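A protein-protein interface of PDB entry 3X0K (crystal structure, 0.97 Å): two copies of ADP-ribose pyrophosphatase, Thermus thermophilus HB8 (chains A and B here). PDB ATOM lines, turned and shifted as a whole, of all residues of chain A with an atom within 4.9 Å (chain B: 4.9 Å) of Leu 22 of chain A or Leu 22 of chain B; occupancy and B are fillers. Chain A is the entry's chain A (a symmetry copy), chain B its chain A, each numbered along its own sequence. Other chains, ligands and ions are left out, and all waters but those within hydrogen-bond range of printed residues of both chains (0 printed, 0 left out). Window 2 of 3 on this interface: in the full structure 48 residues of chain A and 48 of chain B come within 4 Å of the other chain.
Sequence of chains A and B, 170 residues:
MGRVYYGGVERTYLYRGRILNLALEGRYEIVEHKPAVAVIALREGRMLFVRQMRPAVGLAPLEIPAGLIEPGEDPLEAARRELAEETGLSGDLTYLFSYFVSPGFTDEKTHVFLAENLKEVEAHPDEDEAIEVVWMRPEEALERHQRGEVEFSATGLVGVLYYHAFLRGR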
ATOM      1  N   THR A  12     -21.264  10.614  -5.653  1.00  0.00           N
ATOM      2  CA  THR A  12     -20.316   9.574  -5.259  1.00  0.00           C
ATOM      3  C   THR A  12     -19.489  10.082  -4.088  1.00  0.00           C
ATOM      4  O   THR A  12     -19.051  11.251  -4.021  1.00  0.00           O
ATOM      5  CB  THR A  12     -19.425   9.193  -6.431  1.00  0.00           C
ATOM      6  OG1 THR A  12     -18.535  10.285  -6.641  1.00  0.00           O
ATOM      7  CG2 THR A  12     -20.259   9.059  -7.700  1.00  0.00           C
ATOM      8  N   TYR A  13     -19.313   9.225  -3.103  1.00  0.00           N
ATOM      9  CA  TYR A  13     -18.761   9.565  -1.832  1.00  0.00           C
ATOM     10  C   TYR A  13     -17.269   9.307  -1.766  1.00  0.00           C
ATOM     11  O   TYR A  13     -16.793   8.142  -2.060  1.00  0.00           O
ATOM     12  CB  TYR A  13     -19.538   8.809  -0.707  1.00  0.00           C
ATOM     13  CG  TYR A  13     -20.918   9.428  -0.643  1.00  0.00           C
ATOM     14  CD1 TYR A  13     -21.956   8.999  -1.433  1.00  0.00           C
ATOM     15  CD2 TYR A  13     -21.142  10.559   0.194  1.00  0.00           C
ATOM     16  CE1 TYR A  13     -23.198   9.595  -1.384  1.00  0.00           C
ATOM     17  CE2 TYR A  13     -22.392  11.150   0.236  1.00  0.00           C
ATOM     18  CZ  TYR A  13     -23.396  10.673  -0.558  1.00  0.00           C
ATOM     19  OH  TYR A  13     -24.643  11.229  -0.529  1.00  0.00           O
ATOM     20  N   LEU A  14     -16.493  10.292  -1.419  1.00  0.00           N
ATOM     21  CA  LEU A  14     -15.044  10.191  -1.250  1.00  0.00           C
ATOM     22  C   LEU A  14     -14.733   9.944   0.228  1.00  0.00           C
ATOM     23  O   LEU A  14     -13.652   9.395   0.473  1.00  0.00           O
ATOM     24  CB  LEU A  14     -14.281  11.437  -1.691  1.00  0.00           C
ATOM     25  CG  LEU A  14     -14.504  11.883  -3.134  1.00  0.00           C
ATOM     26  CD1 LEU A  14     -13.562  13.024  -3.503  1.00  0.00           C
ATOM     27  CD2 LEU A  14     -14.310  10.703  -4.046  1.00  0.00           C
ATOM     28  N   TYR A  15     -15.608  10.367   1.135  1.00  0.00           N
ATOM     29  CA  TYR A  15     -15.321  10.289   2.561  1.00  0.00           C
ATOM     30  C   TYR A  15     -16.634  10.329   3.339  1.00  0.00           C
ATOM     31  O   TYR A  15     -17.471  11.191   3.052  1.00  0.00           O
ATOM     32  CB  TYR A  15     -14.380  11.462   2.999  1.00  0.00           C
ATOM     33  CG  TYR A  15     -14.117  11.422   4.481  1.00  0.00           C
ATOM     34  CD1 TYR A  15     -13.267  10.525   5.071  1.00  0.00           C
ATOM     35  CD2 TYR A  15     -14.732  12.310   5.366  1.00  0.00           C
ATOM     36  CE1 TYR A  15     -13.015  10.494   6.424  1.00  0.00           C
ATOM     37  CE2 TYR A  15     -14.530  12.311   6.747  1.00  0.00           C
ATOM     38  CZ  TYR A  15     -13.646  11.372   7.287  1.00  0.00           C
ATOM     39  OH  TYR A  15     -13.405  11.317   8.626  1.00  0.00           O
ATOM     40  N   LEU A  20     -19.294  15.075   8.816  1.00  0.00           N
ATOM     41  CA  LEU A  20     -19.437  15.456   7.414  1.00  0.00           C
ATOM     42  C   LEU A  20     -19.169  14.226   6.543  1.00  0.00           C
ATOM     43  O   LEU A  20     -18.479  13.310   6.928  1.00  0.00           O
ATOM     44  CB  LEU A  20     -18.502  16.630   7.036  1.00  0.00           C
ATOM     45  CG  LEU A  20     -16.984  16.462   7.065  1.00  0.00           C
ATOM     46  CD1 LEU A  20     -16.436  15.817   5.794  1.00  0.00           C
ATOM     47  CD2 LEU A  20     -16.273  17.820   7.238  1.00  0.00           C
ATOM     48  N   ASN A  21     -19.712  14.324   5.339  1.00  0.00           N
ATOM     49  CA  ASN A  21     -19.359  13.460   4.218  1.00  0.00           C
ATOM     50  C   ASN A  21     -18.854  14.363   3.084  1.00  0.00           C
ATOM     51  O   ASN A  21     -19.372  15.494   2.904  1.00  0.00           O
ATOM     52  CB  ASN A  21     -20.538  12.665   3.644  1.00  0.00           C
ATOM     53  CG  ASN A  21     -21.209  11.855   4.755  1.00  0.00           C
ATOM     54  OD1 ASN A  21     -20.520  11.257   5.640  1.00  0.00           O
ATOM     55  ND2 ASN A  21     -22.553  11.867   4.690  1.00  0.00           N
ATOM     56  N   LEU A  22     -17.896  13.900   2.287  1.00  0.00           N
ATOM     57  CA  LEU A  22     -17.442  14.583   1.116  1.00  0.00           C
ATOM     58  C   LEU A  22     -17.906  13.763  -0.131  1.00  0.00           C
ATOM     59  O   LEU A  22     -17.620  12.558  -0.212  1.00  0.00           O
ATOM     60  CB  LEU A  22     -15.939  14.734   1.071  1.00  0.00           C
ATOM     61  CG  LEU A  22     -15.399  15.324  -0.234  1.00  0.00           C
ATOM     62  CD1 LEU A  22     -15.902  16.748  -0.493  1.00  0.00           C
ATOM     63  CD2 LEU A  22     -13.872  15.252  -0.104  1.00  0.00           C
ATOM     64  N   ALA A  23     -18.600  14.436  -1.035  1.00  0.00           N
ATOM     65  CA  ALA A  23     -19.164  13.777  -2.214  1.00  0.00           C
ATOM     66  C   ALA A  23     -18.777  14.621  -3.423  1.00  0.00           C
ATOM     67  O   ALA A  23     -18.572  15.836  -3.328  1.00  0.00           O
ATOM     68  CB  ALA A  23     -20.657  13.643  -2.160  1.00  0.00           C
ATOM     69  N   LEU A  24     -18.754  13.956  -4.572  1.00  0.00           N
ATOM     70  CA  LEU A  24     -18.742  14.643  -5.846  1.00  0.00           C
ATOM     71  C   LEU A  24     -20.100  14.419  -6.542  1.00  0.00           C
ATOM     72  O   LEU A  24     -20.675  13.363  -6.518  1.00  0.00           O
ATOM     73  CB  LEU A  24     -17.673  14.070  -6.758  1.00  0.00           C
ATOM     74  CG  LEU A  24     -16.290  14.083  -6.170  1.00  0.00           C
ATOM     75  CD1 LEU A  24     -15.259  13.492  -7.150  1.00  0.00           C
ATOM     76  CD2 LEU A  24     -15.829  15.500  -5.865  1.00  0.00           C
ATOM     77  N   GLU A  29     -18.092  19.668  -5.847  1.00  0.00           N
ATOM     78  CA  GLU A  29     -17.628  19.108  -4.556  1.00  0.00           C
ATOM     79  C   GLU A  29     -18.608  19.563  -3.502  1.00  0.00           C
ATOM     80  O   GLU A  29     -18.869  20.740  -3.336  1.00  0.00           O
ATOM     81  CB  GLU A  29     -16.259  19.678  -4.239  1.00  0.00           C
ATOM     82  CG  GLU A  29     -15.233  19.214  -5.295  1.00  0.00           C
ATOM     83  CD  GLU A  29     -13.966  20.082  -5.364  1.00  0.00           C
ATOM     84  OE1 GLU A  29     -13.936  21.284  -4.856  1.00  0.00           O
ATOM     85  OE2 GLU A  29     -12.972  19.604  -5.924  1.00  0.00           O
ATOM     86  N   ILE A  30     -19.156  18.560  -2.779  1.00  0.00           N
ATOM     87  CA  ILE A  30     -20.248  18.767  -1.860  1.00  0.00           C
ATOM     88  C   ILE A  30     -19.914  18.196  -0.509  1.00  0.00           C
ATOM     89  O   ILE A  30     -19.529  17.030  -0.406  1.00  0.00           O
ATOM     90  CB  ILE A  30     -21.534  18.067  -2.363  1.00  0.00           C
ATOM     91  CG1 ILE A  30     -21.916  18.523  -3.770  1.00  0.00           C
ATOM     92  CG2 ILE A  30     -22.659  18.278  -1.348  1.00  0.00           C
ATOM     93  CD1 ILE A  30     -21.848  20.047  -3.854  1.00  0.00           C
ATOM     94  N   VAL A  31     -20.083  18.997   0.531  1.00  0.00           N
ATOM     95  CA  VAL A  31     -19.902  18.539   1.902  1.00  0.00           C
ATOM     96  C   VAL A  31     -21.283  18.420   2.539  1.00  0.00           C
ATOM     97  O   VAL A  31     -21.933  19.437   2.778  1.00  0.00           O
ATOM     98  CB  VAL A  31     -18.995  19.461   2.685  1.00  0.00           C
ATOM     99  CG1 VAL A  31     -18.864  18.987   4.122  1.00  0.00           C
ATOM    100  CG2 VAL A  31     -17.597  19.494   2.033  1.00  0.00           C
ATOM    101  N   THR B  12      -3.384  16.154   7.819  1.00  0.00           N
ATOM    102  CA  THR B  12      -3.185  15.221   6.713  1.00  0.00           C
ATOM    103  C   THR B  12      -4.368  15.326   5.763  1.00  0.00           C
ATOM    104  O   THR B  12      -5.549  15.433   6.157  1.00  0.00           O
ATOM    105  CB  THR B  12      -3.027  13.801   7.234  1.00  0.00           C
ATOM    106  OG1 THR B  12      -4.312  13.387   7.689  1.00  0.00           O
ATOM    107  CG2 THR B  12      -2.109  13.791   8.451  1.00  0.00           C
ATOM    108  N   TYR B  13      -4.065  15.359   4.481  1.00  0.00           N
ATOM    109  CA  TYR B  13      -4.997  15.671   3.445  1.00  0.00           C
ATOM    110  C   TYR B  13      -5.614  14.427   2.837  1.00  0.00           C
ATOM    111  O   TYR B  13      -4.865  13.485   2.370  1.00  0.00           O
ATOM    112  CB  TYR B  13      -4.300  16.566   2.370  1.00  0.00           C
ATOM    113  CG  TYR B  13      -4.065  17.915   3.016  1.00  0.00           C
ATOM    114  CD1 TYR B  13      -2.939  18.193   3.753  1.00  0.00           C
ATOM    115  CD2 TYR B  13      -5.079  18.913   2.948  1.00  0.00           C
ATOM    116  CE1 TYR B  13      -2.756  19.416   4.360  1.00  0.00           C
ATOM    117  CE2 TYR B  13      -4.886  20.137   3.561  1.00  0.00           C
ATOM    118  CZ  TYR B  13      -3.741  20.369   4.267  1.00  0.00           C
ATOM    119  OH  TYR B  13      -3.517  21.572   4.874  1.00  0.00           O
ATOM    120  N   LEU B  14      -6.913  14.340   2.814  1.00  0.00           N
ATOM    121  CA  LEU B  14      -7.661  13.238   2.210  1.00  0.00           C
ATOM    122  C   LEU B  14      -8.056  13.629   0.784  1.00  0.00           C
ATOM    123  O   LEU B  14      -8.274  12.695   0.003  1.00  0.00           O
ATOM    124  CB  LEU B  14      -8.934  12.867   2.967  1.00  0.00           C
ATOM    125  CG  LEU B  14      -8.754  12.495   4.437  1.00  0.00           C
ATOM    126  CD1 LEU B  14     -10.060  11.979   5.031  1.00  0.00           C
ATOM    127  CD2 LEU B  14      -7.663  11.467   4.552  1.00  0.00           C
ATOM    128  N   TYR B  15      -8.179  14.920   0.496  1.00  0.00           N
ATOM    129  CA  TYR B  15      -8.680  15.366  -0.797  1.00  0.00           C
ATOM    130  C   TYR B  15      -8.226  16.803  -1.042  1.00  0.00           C
ATOM    131  O   TYR B  15      -8.376  17.637  -0.142  1.00  0.00           O
ATOM    132  CB  TYR B  15     -10.242  15.260  -0.850  1.00  0.00           C
ATOM    133  CG  TYR B  15     -10.776  15.766  -2.164  1.00  0.00           C
ATOM    134  CD1 TYR B  15     -10.693  15.058  -3.333  1.00  0.00           C
ATOM    135  CD2 TYR B  15     -11.401  17.009  -2.278  1.00  0.00           C
ATOM    136  CE1 TYR B  15     -11.191  15.512  -4.533  1.00  0.00           C
ATOM    137  CE2 TYR B  15     -11.907  17.528  -3.472  1.00  0.00           C
ATOM    138  CZ  TYR B  15     -11.793  16.754  -4.631  1.00  0.00           C
ATOM    139  OH  TYR B  15     -12.263  17.201  -5.828  1.00  0.00           O
ATOM    140  N   LEU B  20     -12.120  23.319  -2.452  1.00  0.00           N
ATOM    141  CA  LEU B  20     -11.944  22.880  -1.071  1.00  0.00           C
ATOM    142  C   LEU B  20     -10.865  21.795  -1.036  1.00  0.00           C
ATOM    143  O   LEU B  20     -10.621  21.107  -2.000  1.00  0.00           O
ATOM    144  CB  LEU B  20     -13.270  22.379  -0.450  1.00  0.00           C
ATOM    145  CG  LEU B  20     -13.964  21.129  -0.991  1.00  0.00           C
ATOM    146  CD1 LEU B  20     -13.383  19.836  -0.419  1.00  0.00           C
ATOM    147  CD2 LEU B  20     -15.472  21.141  -0.669  1.00  0.00           C
ATOM    148  N   ASN B  21     -10.306  21.670   0.159  1.00  0.00           N
ATOM    149  CA  ASN B  21      -9.490  20.526   0.555  1.00  0.00           C
ATOM    150  C   ASN B  21     -10.153  19.894   1.786  1.00  0.00           C
ATOM    151  O   ASN B  21     -10.719  20.625   2.638  1.00  0.00           O
ATOM    152  CB  ASN B  21      -8.061  20.890   0.972  1.00  0.00           C
ATOM    153  CG  ASN B  21      -7.376  21.676  -0.147  1.00  0.00           C
ATOM    154  OD1 ASN B  21      -7.526  21.348  -1.366  1.00  0.00           O
ATOM    155  ND2 ASN B  21      -6.641  22.713   0.297  1.00  0.00           N
ATOM    156  N   LEU B  22     -10.074  18.577   1.940  1.00  0.00           N
ATOM    157  CA  LEU B  22     -10.526  17.889   3.109  1.00  0.00           C
ATOM    158  C   LEU B  22      -9.269  17.347   3.865  1.00  0.00           C
ATOM    159  O   LEU B  22      -8.446  16.645   3.257  1.00  0.00           O
ATOM    160  CB  LEU B  22     -11.443  16.730   2.791  1.00  0.00           C
ATOM    161  CG  LEU B  22     -11.828  15.874   4.000  1.00  0.00           C
ATOM    162  CD1 LEU B  22     -12.611  16.660   5.056  1.00  0.00           C
ATOM    163  CD2 LEU B  22     -12.631  14.702   3.421  1.00  0.00           C
ATOM    164  N   ALA B  23      -9.170  17.696   5.137  1.00  0.00           N
ATOM    165  CA  ALA B  23      -8.007  17.325   5.945  1.00  0.00           C
ATOM    166  C   ALA B  23      -8.537  16.729   7.243  1.00  0.00           C
ATOM    167  O   ALA B  23      -9.638  17.052   7.704  1.00  0.00           O
ATOM    168  CB  ALA B  23      -7.111  18.485   6.261  1.00  0.00           C
ATOM    169  N   LEU B  24      -7.694  15.905   7.855  1.00  0.00           N
ATOM    170  CA  LEU B  24      -7.881  15.518   9.237  1.00  0.00           C
ATOM    171  C   LEU B  24      -6.772  16.170  10.088  1.00  0.00           C
ATOM    172  O   LEU B  24      -5.633  16.256   9.714  1.00  0.00           O
ATOM    173  CB  LEU B  24      -7.743  14.014   9.400  1.00  0.00           C
ATOM    174  CG  LEU B  24      -8.666  13.213   8.527  1.00  0.00           C
ATOM    175  CD1 LEU B  24      -8.472  11.701   8.747  1.00  0.00           C
ATOM    176  CD2 LEU B  24     -10.125  13.509   8.840  1.00  0.00           C
ATOM    177  N   GLU B  29     -12.212  16.818  11.522  1.00  0.00           N
ATOM    178  CA  GLU B  29     -12.388  16.882  10.052  1.00  0.00           C
ATOM    179  C   GLU B  29     -12.522  18.341   9.689  1.00  0.00           C
ATOM    180  O   GLU B  29     -13.362  19.055  10.206  1.00  0.00           O
ATOM    181  CB  GLU B  29     -13.668  16.160   9.680  1.00  0.00           C
ATOM    182  CG  GLU B  29     -13.551  14.660  10.027  1.00  0.00           C
ATOM    183  CD  GLU B  29     -14.902  13.936  10.148  1.00  0.00           C
ATOM    184  OE1 GLU B  29     -16.015  14.595  10.312  1.00  0.00           O
ATOM    185  OE2 GLU B  29     -14.899  12.701  10.089  1.00  0.00           O
ATOM    186  N   ILE B  30     -11.638  18.768   8.758  1.00  0.00           N
ATOM    187  CA  ILE B  30     -11.477  20.161   8.417  1.00  0.00           C
ATOM    188  C   ILE B  30     -11.591  20.354   6.930  1.00  0.00           C
ATOM    189  O   ILE B  30     -10.904  19.678   6.161  1.00  0.00           O
ATOM    190  CB  ILE B  30     -10.085  20.679   8.854  1.00  0.00           C
ATOM    191  CG1 ILE B  30      -9.838  20.455  10.345  1.00  0.00           C
ATOM    192  CG2 ILE B  30      -9.936  22.147   8.445  1.00  0.00           C
ATOM    193  CD1 ILE B  30     -11.058  20.910  11.144  1.00  0.00           C
ATOM    194  N   VAL B  31     -12.432  21.288   6.516  1.00  0.00           N
ATOM    195  CA  VAL B  31     -12.560  21.653   5.111  1.00  0.00           C
ATOM    196  C   VAL B  31     -11.903  23.018   4.925  1.00  0.00           C
ATOM    197  O   VAL B  31     -12.427  24.018   5.413  1.00  0.00           O
ATOM    198  CB  VAL B  31     -14.002  21.652   4.661  1.00  0.00           C
ATOM    199  CG1 VAL B  31     -14.108  22.084   3.209  1.00  0.00           C
ATOM    200  CG2 VAL B  31     -14.596  20.236   4.814  1.00  0.00           C
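OH of Tyr 15 of chain B sits at hydrogen-bond distance from OE2 of Glu 29 of chain A, at 2.5 Å. The side-chain hydroxyl of Tyr 15 of chain A sits at hydrogen-bond distance from the side-chain carboxylate of Glu 29 of chain B (2.5 Å).
N of Leu 14 of chain B sits at hydrogen-bond distance from O of Leu 22 of chain B (2.8 Å). O of Thr 12 of chain A sits at hydrogen-bond distance from N of Leu 24 of chain A (2.8 Å). The backbone carbonyl oxygen (O) of Thr 12 of chain B sits at hydrogen-bond distance from the backbone NH (N) of Leu 24 of chain B, at 2.8 Å. O of Tyr 15 of chain B sits at hydrogen-bond distance from N of Leu 22 of chain B, 2.8 Å away. N of Leu 14 of chain A lies within hydrogen-bond range of O of Leu 22 of chain A, at 2.8 Å. The backbone NH (N) of Leu 22 of chain A is in hydrogen-bond range of the backbone carbonyl oxygen (O) of Tyr 15 of chain A (2.8 Å).
Leu 14 of chain A touches Tyr 15 of chain B. CD2 of Leu 24 of chain B touches OH of Tyr 15 of chain A (3.95 Å). Leu 20 of chain A touches Leu 22 of chain B. N of Leu 20 of chain A touches OE1 of Glu 29 of chain B (3.6 Å). CD2 of Leu 20 of chain A touches CG2 of Val 31 of chain B, 3.8 Å away. CD2 of Leu 22 of chain A touches CB of Tyr 15 of chain B, at 3.7 Å. Leu 22 of chain A touches Leu 20 of chain B. OH of Tyr 15 of chain B touches CD2 of Leu 24 of chain A, 3.95 Å away. N of Leu 20 of chain B touches OE1 of Glu 29 of chain A (3.6 Å). Leu 20 of chain B touches Val 31 of chain A.
Of the printed residues of chain B, Leu 22 of chain A touches Tyr 15 (3.7 Å), Leu 20 (3.99 Å) and Leu 22 (3.8 Å). Of the printed residues of chain A, Leu 22 of chain B touches Tyr 15, Leu 20 and Leu 22. Of the printed residues of chain A, Tyr 15 of chain B touches Leu 14 (3.5 Å), Leu 22 (3.7 Å), Leu 24 (3.95 Å) and Glu 29 (2.5 Å). Printed residues of chain B within 4 Å of Glu 29 of chain A: Tyr 15 and Leu 20. Printed residues of chain A within 4 Å of Leu 14 of chain B: Tyr 15 (3.5 Å). Of the printed residues of chain B, Leu 14 of chain A touches Tyr 15. Of the printed residues of chain A, Leu 20 of chain B touches Leu 22 (3.99 Å), Glu 29 (3.6 Å) and Val 31 (3.8 Å). Asn 21 of chain B touches none of the printed residues of chain A. The nearest printed residue of chain B that does not touch Leu 22 of chain A is Leu 14 of chain B (6.1 Å). The nearest printed residue of chain A that does not touch Val 31 of chain B is Val 31 of chain A (4.2 Å).
Of the 12 printed residues of chain A, 7 touch a printed residue of chain B. Hydrophobic or aromatic side chains of chain A within 4 Å of the printed part of chain B: Leu 14, Tyr 15, Leu 20, Leu 22, Leu 24 and Val 31. Of the 12 printed residues of chain B, 7 touch a printed residue of chain A. Hydrophobic or aromatic side chains of chain B that line the printed part of chain A: Leu 14, Tyr 15, Leu 20, Leu 22, Leu 24 and Val 31. Along chain B the printed residues that touch a printed residue of chain A span positions 14 to 31. Among the printed residues, no Asp or Glu carboxylate lies within 4 Å of a Lys or Arg side-chain nitrogen of the other chain.
Leu 14 of chain A touches Tyr 15 of chain B, and with the chains exchanged Tyr 15 of chain A touches Leu 14 of chain B. Tyr 15 of chain A touches Glu 29 of chain B, and with the chains exchanged Glu 29 of chain A touches Tyr 15 of chain B. Leu 20 of chain A touches Glu 29 of chain B, and with the chains exchanged Glu 29 of chain A touches Leu 20 of chain B. Leu 20 of chain A touches Val 31 of chain B, and with the chains exchanged Val 31 of chain A touches Leu 20 of chain B. Positions printed for both chains: 12, 13, 14, 15, 20, 21, 22, 23, 24, 29, 30 and 31. Of the 15 pairs that touch across the chains among the printed residues, 15 have their exchanged pair printed and touching as well.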
